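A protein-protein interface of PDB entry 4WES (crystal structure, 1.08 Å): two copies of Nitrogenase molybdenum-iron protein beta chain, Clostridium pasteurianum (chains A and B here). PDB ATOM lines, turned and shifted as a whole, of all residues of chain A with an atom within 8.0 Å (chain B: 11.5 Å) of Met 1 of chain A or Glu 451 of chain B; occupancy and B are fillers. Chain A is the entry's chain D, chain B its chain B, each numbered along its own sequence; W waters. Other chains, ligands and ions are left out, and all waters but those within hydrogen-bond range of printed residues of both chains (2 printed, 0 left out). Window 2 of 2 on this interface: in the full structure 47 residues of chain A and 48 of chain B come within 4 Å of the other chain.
The backbone carbonyl oxygen (O) of Ile 445 of chain B sits close to the side-chain sulfur (SG) of Cys 449 of chain B (3.5 Å).
O of Glu 446 of chain B is in hydrogen-bond range of SG of Cys 449 of chain B (3.8 Å).
The guanidinium group (NE) of Arg 458 of chain B lies within salt-bridge range of the side-chain carboxylate (OE1) of Glu 446 of chain B, at 2.9 Å.
The side-chain carboxylate (OD1) of Asp 3 of chain A is in hydrogen-bond range of the backbone NH (N) of Met 1 of chain A.
The backbone NH (N) of Met 1 of chain A sits at hydrogen-bond distance from the side-chain carboxylate (OE1) of Glu 401 of chain A.
Met 1 of chain A touches Phe 454 of chain B (CE to CG, 3.5 Å).
Lys 396 of chain A touches Phe 454 of chain B (CG to CE2, 3.7 Å).
CD2 of Phe 454 of chain B touches CE1 of Phe 397 of chain A, at 3.5 Å.
Val 456 of chain B touches Phe 397 of chain A (CG2 to CZ, 3.7 Å).
Arg 400 of chain A touches Glu 451 of chain B.
Arg 400 of chain A touches Phe 454 of chain B.
Of the 15 printed residues of chain A, 4 touch a printed residue of chain B.
Of the 15 printed residues of chain B, 7 touch a printed residue of chain A.
Among the printed residues, 13 pairs touch across the chains.
Among the printed residues, Asp or Glu carboxylates within 4 Å of a Lys or Arg side-chain nitrogen of the other chain: Lys 396 of chain A with Glu 446 of chain B.
OE1 of Glu 446 of chain B is in salt-bridge range of NZ of Lys 396 of chain A, at 2.7 Å.
The backbone carbonyl oxygen (O) of Glu 446 of chain B is in hydrogen-bond range of the guanidinium group (NH1) of Arg 400 of chain A, 2.9 Å away.
The backbone carbonyl oxygen (O) of Arg 447 of chain B sits at hydrogen-bond distance from the guanidinium group (NH1) of Arg 400 of chain A, 3.5 Å away.
The guanidinium group of Arg 400 of chain A sits at hydrogen-bond distance from the backbone carbonyl oxygen of Cys 449 of chain B (2.9 Å).
The side-chain carboxylate (OE2) of Glu 451 of chain B is in hydrogen-bond range of the backbone NH (N) of Met 1 of chain A (2.8 Å).
The side-chain amino group (NZ) of Lys 396 of chain A sits at hydrogen-bond distance from the backbone carbonyl oxygen (O) of Glu 455 of chain B (2.8 Å).
The side-chain amino group (NZ) of Lys 396 of chain A is in hydrogen-bond range of the backbone carbonyl oxygen (O) of Val 456 of chain B, 3.0 Å away.
Met 1 of chain A touches just these residues of chain B: Glu 451 (2.8 Å) and Phe 454 (3.5 Å).
Leu 2 of chain A touches none of the printed residues of chain B.
No residue of chain B comes within 4 Å of Asp 3 of chain A.
Of the printed residues of chain B, Lys 396 of chain A touches Glu 446, Phe 454, Glu 455 and Val 456.
Phe 397 of chain A touches two residues of chain B.
No residue of chain B comes within 4 Å of Glu 401 of chain A.
Of the printed residues of chain A, Arg 447 of chain B touches Arg 400.
Thr 450 of chain B touches none of the printed residues of chain A.
Glu 451 of chain B touches two residues of chain A.
The nearest residue of chain B that does not touch Met 1 of chain A is Thr 450 of chain B (5.8 Å).
The nearest printed residue of chain A that does not touch Val 456 of chain B is Gly 395 of chain A (8.4 Å).
No position is printed for both chains.
Of the 13 pairs that touch across the chains among the printed residues, none has its exchanged pair printed and touching as well.
Water W2 bridges OE1 of Glu 451 of chain B (2.7 Å) and OD2 of Asp 3 of chain A (2.8 Å).
Water W1 lies within hydrogen-bond range of the side-chain carboxylate of Glu 451 of chain B and the guanidinium group of Arg 400 of chain A.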
ATOM      1  N   MET A   1       0.317   4.736  -1.667  1.00  0.00           N
ATOM      2  CA  MET A   1       0.306   5.348  -3.023  1.00  0.00           C
ATOM      3  C   MET A   1       1.378   4.616  -3.826  1.00  0.00           C
ATOM      4  O   MET A   1       2.394   4.184  -3.286  1.00  0.00           O
ATOM      5  CB  MET A   1       0.584   6.846  -2.872  1.00  0.00           C
ATOM      6  CG  MET A   1       0.732   7.605  -4.161  1.00  0.00           C
ATOM      7  SD  MET A   1       0.567   9.386  -3.956  1.00  0.00           S
ATOM      8  CE  MET A   1      -1.223   9.499  -3.707  1.00  0.00           C
ATOM      9  N   LEU A   2       1.132   4.464  -5.134  1.00  0.00           N
ATOM     10  CA  LEU A   2       2.051   3.689  -5.982  1.00  0.00           C
ATOM     11  C   LEU A   2       2.303   2.325  -5.354  1.00  0.00           C
ATOM     12  O   LEU A   2       3.419   1.792  -5.305  1.00  0.00           O
ATOM     13  CB  LEU A   2       3.350   4.454  -6.256  1.00  0.00           C
ATOM     14  CG  LEU A   2       3.197   5.718  -7.118  1.00  0.00           C
ATOM     15  CD1 LEU A   2       4.452   6.580  -7.031  1.00  0.00           C
ATOM     16  CD2 LEU A   2       2.899   5.380  -8.554  1.00  0.00           C
ATOM     17  N   ASP A   3       1.218   1.709  -4.888  1.00  0.00           N
ATOM     18  CA  ASP A   3       1.332   0.494  -4.094  1.00  0.00           C
ATOM     19  C   ASP A   3       1.871  -0.673  -4.888  1.00  0.00           C
ATOM     20  O   ASP A   3       2.436  -1.598  -4.296  1.00  0.00           O
ATOM     21  CB  ASP A   3      -0.002   0.112  -3.472  1.00  0.00           C
ATOM     22  CG  ASP A   3      -0.456   1.080  -2.393  1.00  0.00           C
ATOM     23  OD1 ASP A   3       0.250   2.019  -2.023  1.00  0.00           O
ATOM     24  OD2 ASP A   3      -1.595   0.879  -1.907  1.00  0.00           O
ATOM     25  N   ALA A   4       1.662  -0.658  -6.194  1.00  0.00           N
ATOM     26  CA  ALA A   4       2.067  -1.760  -7.059  1.00  0.00           C
ATOM     27  C   ALA A   4       3.553  -1.764  -7.408  1.00  0.00           C
ATOM     28  O   ALA A   4       4.011  -2.671  -8.099  1.00  0.00           O
ATOM     29  CB  ALA A   4       1.249  -1.733  -8.334  1.00  0.00           C
ATOM     30  N   THR A   5       4.297  -0.725  -6.985  1.00  0.00           N
ATOM     31  CA  THR A   5       5.731  -0.653  -7.324  1.00  0.00           C
ATOM     32  C   THR A   5       6.549  -1.455  -6.328  1.00  0.00           C
ATOM     33  O   THR A   5       6.614  -1.094  -5.162  1.00  0.00           O
ATOM     34  CB  THR A   5       6.170   0.792  -7.320  1.00  0.00           C
ATOM     35  OG1 THR A   5       5.356   1.487  -8.268  1.00  0.00           O
ATOM     36  CG2 THR A   5       7.639   0.933  -7.687  1.00  0.00           C
ATOM     37  N   HIS A 378      11.591   5.445  -8.389  1.00  0.00           N
ATOM     38  CA  HIS A 378      10.877   5.016  -7.195  1.00  0.00           C
ATOM     39  C   HIS A 378      11.474   3.718  -6.640  1.00  0.00           C
ATOM     40  O   HIS A 378      11.711   3.605  -5.421  1.00  0.00           O
ATOM     41  CB  HIS A 378       9.403   4.886  -7.467  1.00  0.00           C
ATOM     42  CG  HIS A 378       8.592   4.745  -6.218  1.00  0.00           C
ATOM     43  ND1 HIS A 378       7.265   4.405  -6.254  1.00  0.00           N
ATOM     44  CD2 HIS A 378       8.930   4.909  -4.912  1.00  0.00           C
ATOM     45  CE1 HIS A 378       6.813   4.350  -5.011  1.00  0.00           C
ATOM     46  NE2 HIS A 378       7.791   4.666  -4.179  1.00  0.00           N
ATOM     47  N   LYS A 382      13.160   3.115  -2.884  1.00  0.00           N
ATOM     48  CA  LYS A 382      12.733   2.085  -1.935  1.00  0.00           C
ATOM     49  C   LYS A 382      13.910   1.308  -1.379  1.00  0.00           C
ATOM     50  O   LYS A 382      13.834   0.775  -0.277  1.00  0.00           O
ATOM     51  CB  LYS A 382      11.736   1.143  -2.550  1.00  0.00           C
ATOM     52  CG  LYS A 382      10.401   1.785  -2.793  1.00  0.00           C
ATOM     53  CD  LYS A 382       9.339   0.762  -3.138  1.00  0.00           C
ATOM     54  CE  LYS A 382       7.951   1.389  -3.197  1.00  0.00           C
ATOM     55  NZ  LYS A 382       6.848   0.436  -2.846  1.00  0.00           N
ATOM     56  N   GLY A 395       6.493  13.633 -10.271  1.00  0.00           N
ATOM     57  CA  GLY A 395       7.217  13.250  -9.084  1.00  0.00           C
ATOM     58  C   GLY A 395       6.423  13.372  -7.799  1.00  0.00           C
ATOM     59  O   GLY A 395       6.805  12.788  -6.793  1.00  0.00           O
ATOM     60  N   LYS A 396       5.306  14.087  -7.826  1.00  0.00           N
ATOM     61  CA  LYS A 396       4.531  14.373  -6.606  1.00  0.00           C
ATOM     62  C   LYS A 396       4.032  13.060  -5.987  1.00  0.00           C
ATOM     63  O   LYS A 396       3.843  12.978  -4.760  1.00  0.00           O
ATOM     64  CB  LYS A 396       3.317  15.297  -6.864  1.00  0.00           C
ATOM     65  CG  LYS A 396       2.197  14.707  -7.716  1.00  0.00           C
ATOM     66  CD  LYS A 396       1.170  15.616  -8.413  1.00  0.00           C
ATOM     67  CE  LYS A 396       0.250  16.267  -7.498  1.00  0.00           C
ATOM     68  NZ  LYS A 396      -0.526  17.327  -8.132  1.00  0.00           N
ATOM     69  N   PHE A 397       3.793  12.040  -6.806  1.00  0.00           N
ATOM     70  CA  PHE A 397       3.313  10.770  -6.304  1.00  0.00           C
ATOM     71  C   PHE A 397       4.370  10.065  -5.467  1.00  0.00           C
ATOM     72  O   PHE A 397       4.089   9.467  -4.407  1.00  0.00           O
ATOM     73  CB  PHE A 397       2.854   9.858  -7.441  1.00  0.00           C
ATOM     74  CG  PHE A 397       1.664  10.343  -8.202  1.00  0.00           C
ATOM     75  CD1 PHE A 397       0.375   9.888  -7.871  1.00  0.00           C
ATOM     76  CD2 PHE A 397       1.772  11.251  -9.245  1.00  0.00           C
ATOM     77  CE1 PHE A 397      -0.735  10.295  -8.579  1.00  0.00           C
ATOM     78  CE2 PHE A 397       0.663  11.639  -9.957  1.00  0.00           C
ATOM     79  CZ  PHE A 397      -0.598  11.184  -9.614  1.00  0.00           C
ATOM     80  N   ILE A 398       5.606  10.085  -5.954  1.00  0.00           N
ATOM     81  CA  ILE A 398       6.725   9.550  -5.201  1.00  0.00           C
ATOM     82  C   ILE A 398       6.972  10.364  -3.938  1.00  0.00           C
ATOM     83  O   ILE A 398       7.227   9.826  -2.852  1.00  0.00           O
ATOM     84  CB  ILE A 398       8.006   9.482  -6.078  1.00  0.00           C
ATOM     85  CG1 ILE A 398       7.795   8.607  -7.311  1.00  0.00           C
ATOM     86  CG2 ILE A 398       9.189   9.008  -5.270  1.00  0.00           C
ATOM     87  CD1 ILE A 398       8.933   8.679  -8.296  1.00  0.00           C
ATOM     88  N   ALA A 399       6.952  11.693  -4.082  1.00  0.00           N
ATOM     89  CA  ALA A 399       7.183  12.563  -2.938  1.00  0.00           C
ATOM     90  C   ALA A 399       6.203  12.273  -1.799  1.00  0.00           C
ATOM     91  O   ALA A 399       6.609  12.272  -0.639  1.00  0.00           O
ATOM     92  CB  ALA A 399       7.081  14.020  -3.357  1.00  0.00           C
ATOM     93  N   ARG A 400       4.934  12.118  -2.145  1.00  0.00           N
ATOM     94  CA  ARG A 400       3.953  11.787  -1.107  1.00  0.00           C
ATOM     95  C   ARG A 400       4.160  10.391  -0.558  1.00  0.00           C
ATOM     96  O   ARG A 400       4.175  10.212   0.679  1.00  0.00           O
ATOM     97  CB  ARG A 400       2.535  11.958  -1.645  1.00  0.00           C
ATOM     98  CG  ARG A 400       1.501  11.420  -0.653  1.00  0.00           C
ATOM     99  CD  ARG A 400       0.135  11.969  -0.851  1.00  0.00           C
ATOM    100  NE  ARG A 400      -0.827  11.191  -0.074  1.00  0.00           N
ATOM    101  CZ  ARG A 400      -2.041  11.569   0.245  1.00  0.00           C
ATOM    102  NH1 ARG A 400      -2.490  12.749  -0.100  1.00  0.00           N
ATOM    103  NH2 ARG A 400      -2.831  10.719   0.887  1.00  0.00           N
ATOM    104  N   GLU A 401       4.299   9.395  -1.399  1.00  0.00           N
ATOM    105  CA  GLU A 401       4.440   8.028  -0.920  1.00  0.00           C
ATOM    106  C   GLU A 401       5.638   7.866  -0.005  1.00  0.00           C
ATOM    107  O   GLU A 401       5.572   7.152   0.995  1.00  0.00           O
ATOM    108  CB  GLU A 401       4.513   7.049  -2.104  1.00  0.00           C
ATOM    109  CG  GLU A 401       4.862   5.632  -1.735  1.00  0.00           C
ATOM    110  CD  GLU A 401       3.867   4.916  -0.862  1.00  0.00           C
ATOM    111  OE1 GLU A 401       2.799   5.473  -0.495  1.00  0.00           O
ATOM    112  OE2 GLU A 401       4.140   3.717  -0.577  1.00  0.00           O
ATOM    113  N   GLU A 402       6.763   8.491  -0.374  1.00  0.00           N
ATOM    114  CA  GLU A 402       8.026   8.300   0.322  1.00  0.00           C
ATOM    115  C   GLU A 402       8.370   9.430   1.274  1.00  0.00           C
ATOM    116  O   GLU A 402       9.393   9.349   1.959  1.00  0.00           O
ATOM    117  CB  GLU A 402       9.159   8.087  -0.692  1.00  0.00           C
ATOM    118  CG  GLU A 402       8.961   6.895  -1.608  1.00  0.00           C
ATOM    119  CD  GLU A 402       8.933   5.549  -0.918  1.00  0.00           C
ATOM    120  OE1 GLU A 402       9.581   5.395   0.140  1.00  0.00           O
ATOM    121  OE2 GLU A 402       8.251   4.625  -1.434  1.00  0.00           O
ATOM    122  N   ASP B 443      -0.346  22.850  -1.200  1.00  0.00           N
ATOM    123  CA  ASP B 443       0.489  21.887  -0.514  1.00  0.00           C
ATOM    124  C   ASP B 443      -0.315  21.155   0.566  1.00  0.00           C
ATOM    125  O   ASP B 443      -0.212  19.930   0.723  1.00  0.00           O
ATOM    126  CB  ASP B 443       1.689  22.578   0.148  1.00  0.00           C
ATOM    127  CG  ASP B 443       2.864  22.853  -0.793  1.00  0.00           C
ATOM    128  OD1 ASP B 443       2.890  22.360  -1.935  1.00  0.00           O
ATOM    129  OD2 ASP B 443       3.753  23.592  -0.322  1.00  0.00           O
ATOM    130  N   LYS B 444      -1.107  21.893   1.340  1.00  0.00           N
ATOM    131  CA  LYS B 444      -1.911  21.272   2.392  1.00  0.00           C
ATOM    132  C   LYS B 444      -2.959  20.357   1.774  1.00  0.00           C
ATOM    133  O   LYS B 444      -3.138  19.238   2.232  1.00  0.00           O
ATOM    134  CB  LYS B 444      -2.556  22.322   3.284  1.00  0.00           C
ATOM    135  CG  LYS B 444      -3.459  21.681   4.364  1.00  0.00           C
ATOM    136  CD  LYS B 444      -4.051  22.674   5.312  1.00  0.00           C
ATOM    137  CE  LYS B 444      -5.030  21.920   6.254  1.00  0.00           C
ATOM    138  NZ  LYS B 444      -5.610  22.759   7.292  1.00  0.00           N
ATOM    139  N   ILE B 445      -3.669  20.815   0.743  1.00  0.00           N
ATOM    140  CA  ILE B 445      -4.692  19.997   0.109  1.00  0.00           C
ATOM    141  C   ILE B 445      -4.112  18.665  -0.326  1.00  0.00           C
ATOM    142  O   ILE B 445      -4.691  17.595  -0.071  1.00  0.00           O
ATOM    143  CB  ILE B 445      -5.317  20.729  -1.100  1.00  0.00           C
ATOM    144  CG1 ILE B 445      -6.155  21.904  -0.633  1.00  0.00           C
ATOM    145  CG2 ILE B 445      -6.124  19.768  -1.972  1.00  0.00           C
ATOM    146  CD1 ILE B 445      -6.581  22.843  -1.735  1.00  0.00           C
ATOM    147  N   GLU B 446      -2.939  18.704  -0.960  1.00  0.00           N
ATOM    148  CA  GLU B 446      -2.359  17.497  -1.560  1.00  0.00           C
ATOM    149  C   GLU B 446      -1.697  16.587  -0.534  1.00  0.00           C
ATOM    150  O   GLU B 446      -1.580  15.388  -0.768  1.00  0.00           O
ATOM    151  CB  GLU B 446      -1.400  17.883  -2.690  1.00  0.00           C
ATOM    152  CG  GLU B 446      -2.137  18.689  -3.768  1.00  0.00           C
ATOM    153  CD  GLU B 446      -1.439  18.684  -5.098  1.00  0.00           C
ATOM    154  OE1 GLU B 446      -2.082  18.239  -6.101  1.00  0.00           O
ATOM    155  OE2 GLU B 446      -0.260  19.029  -5.168  1.00  0.00           O
ATOM    156  N   ARG B 447      -1.282  17.144   0.603  1.00  0.00           N
ATOM    157  CA  ARG B 447      -0.754  16.302   1.679  1.00  0.00           C
ATOM    158  C   ARG B 447      -1.889  15.591   2.422  1.00  0.00           C
ATOM    159  O   ARG B 447      -1.724  14.449   2.841  1.00  0.00           O
ATOM    160  CB  ARG B 447       0.061  17.120   2.682  1.00  0.00           C
ATOM    161  CG  ARG B 447       0.993  16.297   3.550  1.00  0.00           C
ATOM    162  CD  ARG B 447       1.755  17.155   4.548  1.00  0.00           C
ATOM    163  NE  ARG B 447       2.319  18.349   3.928  1.00  0.00           N
ATOM    164  CZ  ARG B 447       1.854  19.588   4.104  1.00  0.00           C
ATOM    165  NH1 ARG B 447       0.800  19.791   4.882  1.00  0.00           N
ATOM    166  NH2 ARG B 447       2.424  20.633   3.502  1.00  0.00           N
ATOM    167  N   GLU B 448      -3.034  16.241   2.569  1.00  0.00           N
ATOM    168  CA  GLU B 448      -4.087  15.739   3.446  1.00  0.00           C
ATOM    169  C   GLU B 448      -5.195  15.016   2.743  1.00  0.00           C
ATOM    170  O   GLU B 448      -5.985  14.316   3.398  1.00  0.00           O
ATOM    171  CB  GLU B 448      -4.678  16.870   4.266  1.00  0.00           C
ATOM    172  CG  GLU B 448      -3.620  17.462   5.133  1.00  0.00           C
ATOM    173  CD  GLU B 448      -4.116  18.347   6.198  1.00  0.00           C
ATOM    174  OE1 GLU B 448      -3.294  18.658   7.099  1.00  0.00           O
ATOM    175  OE2 GLU B 448      -5.291  18.741   6.089  1.00  0.00           O
ATOM    176  N   CYS B 449      -5.325  15.129   1.422  1.00  0.00           N
ATOM    177  CA  CYS B 449      -6.396  14.453   0.744  1.00  0.00           C
ATOM    178  C   CYS B 449      -6.232  12.941   0.813  1.00  0.00           C
ATOM    179  O   CYS B 449      -5.129  12.437   0.998  1.00  0.00           O
ATOM    180  CB  CYS B 449      -6.527  14.908  -0.706  1.00  0.00           C
ATOM    181  SG  CYS B 449      -5.130  14.529  -1.763  1.00  0.00           S
ATOM    182  N   THR B 450      -7.338  12.213   0.670  1.00  0.00           N
ATOM    183  CA  THR B 450      -7.231  10.772   0.558  1.00  0.00           C
ATOM    184  C   THR B 450      -6.483  10.425  -0.741  1.00  0.00           C
ATOM    185  O   THR B 450      -6.415  11.220  -1.696  1.00  0.00           O
ATOM    186  CB  THR B 450      -8.609  10.131   0.537  1.00  0.00           C
ATOM    187  OG1 THR B 450      -9.302  10.618  -0.604  1.00  0.00           O
ATOM    188  CG2 THR B 450      -9.374  10.425   1.819  1.00  0.00           C
ATOM    189  N   GLU B 451      -5.947   9.219  -0.820  1.00  0.00           N
ATOM    190  CA  GLU B 451      -5.227   8.825  -2.038  1.00  0.00           C
ATOM    191  C   GLU B 451      -6.126   8.860  -3.251  1.00  0.00           C
ATOM    192  O   GLU B 451      -5.685   9.265  -4.325  1.00  0.00           O
ATOM    193  CB  GLU B 451      -4.589   7.443  -1.894  1.00  0.00           C
ATOM    194  CG  GLU B 451      -3.467   7.428  -0.878  1.00  0.00           C
ATOM    195  CD  GLU B 451      -2.559   6.211  -0.983  1.00  0.00           C
ATOM    196  OE1 GLU B 451      -2.788   5.360  -1.879  1.00  0.00           O
ATOM    197  OE2 GLU B 451      -1.597   6.130  -0.194  1.00  0.00           O
ATOM    198  N   GLU B 452      -7.389   8.470  -3.083  1.00  0.00           N
ATOM    199  CA  GLU B 452      -8.272   8.418  -4.234  1.00  0.00           C
ATOM    200  C   GLU B 452      -8.618   9.824  -4.728  1.00  0.00           C
ATOM    201  O   GLU B 452      -9.068   9.992  -5.880  1.00  0.00           O
ATOM    202  CB  GLU B 452      -9.539   7.603  -3.957  1.00  0.00           C
ATOM    203  CG  GLU B 452     -10.463   8.157  -2.893  1.00  0.00           C
ATOM    204  CD  GLU B 452     -10.171   7.647  -1.477  1.00  0.00           C
ATOM    205  OE1 GLU B 452      -9.025   7.210  -1.181  1.00  0.00           O
ATOM    206  OE2 GLU B 452     -11.100   7.706  -0.646  1.00  0.00           O
ATOM    207  N   ASP B 453      -8.436  10.828  -3.875  1.00  0.00           N
ATOM    208  CA  ASP B 453      -8.683  12.232  -4.231  1.00  0.00           C
ATOM    209  C   ASP B 453      -7.444  12.961  -4.696  1.00  0.00           C
ATOM    210  O   ASP B 453      -7.487  14.172  -4.993  1.00  0.00           O
ATOM    211  CB  ASP B 453      -9.303  12.981  -3.029  1.00  0.00           C
ATOM    212  CG  ASP B 453     -10.736  12.601  -2.754  1.00  0.00           C
ATOM    213  OD1 ASP B 453     -11.370  12.033  -3.647  1.00  0.00           O
ATOM    214  OD2 ASP B 453     -11.200  12.894  -1.635  1.00  0.00           O
ATOM    215  N   PHE B 454      -6.321  12.249  -4.805  1.00  0.00           N
ATOM    216  CA  PHE B 454      -5.076  12.884  -5.223  1.00  0.00           C
ATOM    217  C   PHE B 454      -5.187  13.106  -6.737  1.00  0.00           C
ATOM    218  O   PHE B 454      -5.791  12.303  -7.482  1.00  0.00           O
ATOM    219  CB  PHE B 454      -3.929  11.959  -4.832  1.00  0.00           C
ATOM    220  CG  PHE B 454      -2.564  12.577  -4.847  1.00  0.00           C
ATOM    221  CD1 PHE B 454      -2.107  13.350  -3.765  1.00  0.00           C
ATOM    222  CD2 PHE B 454      -1.699  12.350  -5.898  1.00  0.00           C
ATOM    223  CE1 PHE B 454      -0.837  13.896  -3.761  1.00  0.00           C
ATOM    224  CE2 PHE B 454      -0.422  12.860  -5.885  1.00  0.00           C
ATOM    225  CZ  PHE B 454       0.018  13.616  -4.818  1.00  0.00           C
ATOM    226  N   GLU B 455      -4.676  14.248  -7.174  1.00  0.00           N
ATOM    227  CA  GLU B 455      -4.852  14.801  -8.542  1.00  0.00           C
ATOM    228  C   GLU B 455      -3.510  15.022  -9.218  1.00  0.00           C
ATOM    229  O   GLU B 455      -2.556  15.405  -8.558  1.00  0.00           O
ATOM    230  CB  GLU B 455      -5.489  16.197  -8.402  1.00  0.00           C
ATOM    231  CG  GLU B 455      -6.834  16.276  -7.741  1.00  0.00           C
ATOM    232  CD  GLU B 455      -7.959  15.626  -8.496  1.00  0.00           C
ATOM    233  OE1 GLU B 455      -7.832  15.312  -9.715  1.00  0.00           O
ATOM    234  OE2 GLU B 455      -9.037  15.413  -7.888  1.00  0.00           O
ATOM    235  N   VAL B 456      -3.469  14.849 -10.534  1.00  0.00           N
ATOM    236  CA  VAL B 456      -2.319  15.344 -11.330  1.00  0.00           C
ATOM    237  C   VAL B 456      -2.407  16.857 -11.494  1.00  0.00           C
ATOM    238  O   VAL B 456      -1.641  17.587 -10.884  1.00  0.00           O
ATOM    239  CB  VAL B 456      -2.180  14.628 -12.688  1.00  0.00           C
ATOM    240  CG1 VAL B 456      -1.109  15.259 -13.522  1.00  0.00           C
ATOM    241  CG2 VAL B 456      -1.862  13.171 -12.472  1.00  0.00           C
ATOM    242  N   ARG B 458      -3.877  20.693 -11.154  1.00  0.00           N
ATOM    243  CA  ARG B 458      -4.633  21.571 -10.241  1.00  0.00           C
ATOM    244  C   ARG B 458      -4.767  22.938 -10.875  1.00  0.00           C
ATOM    245  O   ARG B 458      -5.608  23.740 -10.383  1.00  0.00           O
ATOM    246  CB  ARG B 458      -3.924  21.750  -8.889  1.00  0.00           C
ATOM    247  CG  ARG B 458      -3.809  20.473  -8.057  1.00  0.00           C
ATOM    248  CD  ARG B 458      -5.074  20.156  -7.343  1.00  0.00           C
ATOM    249  NE  ARG B 458      -4.853  19.058  -6.394  1.00  0.00           N
ATOM    250  CZ  ARG B 458      -5.782  18.590  -5.582  1.00  0.00           C
ATOM    251  NH1 ARG B 458      -6.984  19.143  -5.574  1.00  0.00           N
ATOM    252  NH2 ARG B 458      -5.514  17.549  -4.780  1.00  0.00           N
ATOM    253  OXT ARG B 458      -4.009  23.227 -11.837  1.00  0.00           O
HETATM  254  O   HOH W   1      -0.411   8.474   0.676  1.00  0.00           O
HETATM  255  O   HOH W   2      -3.669   2.779  -1.887  1.00  0.00           O
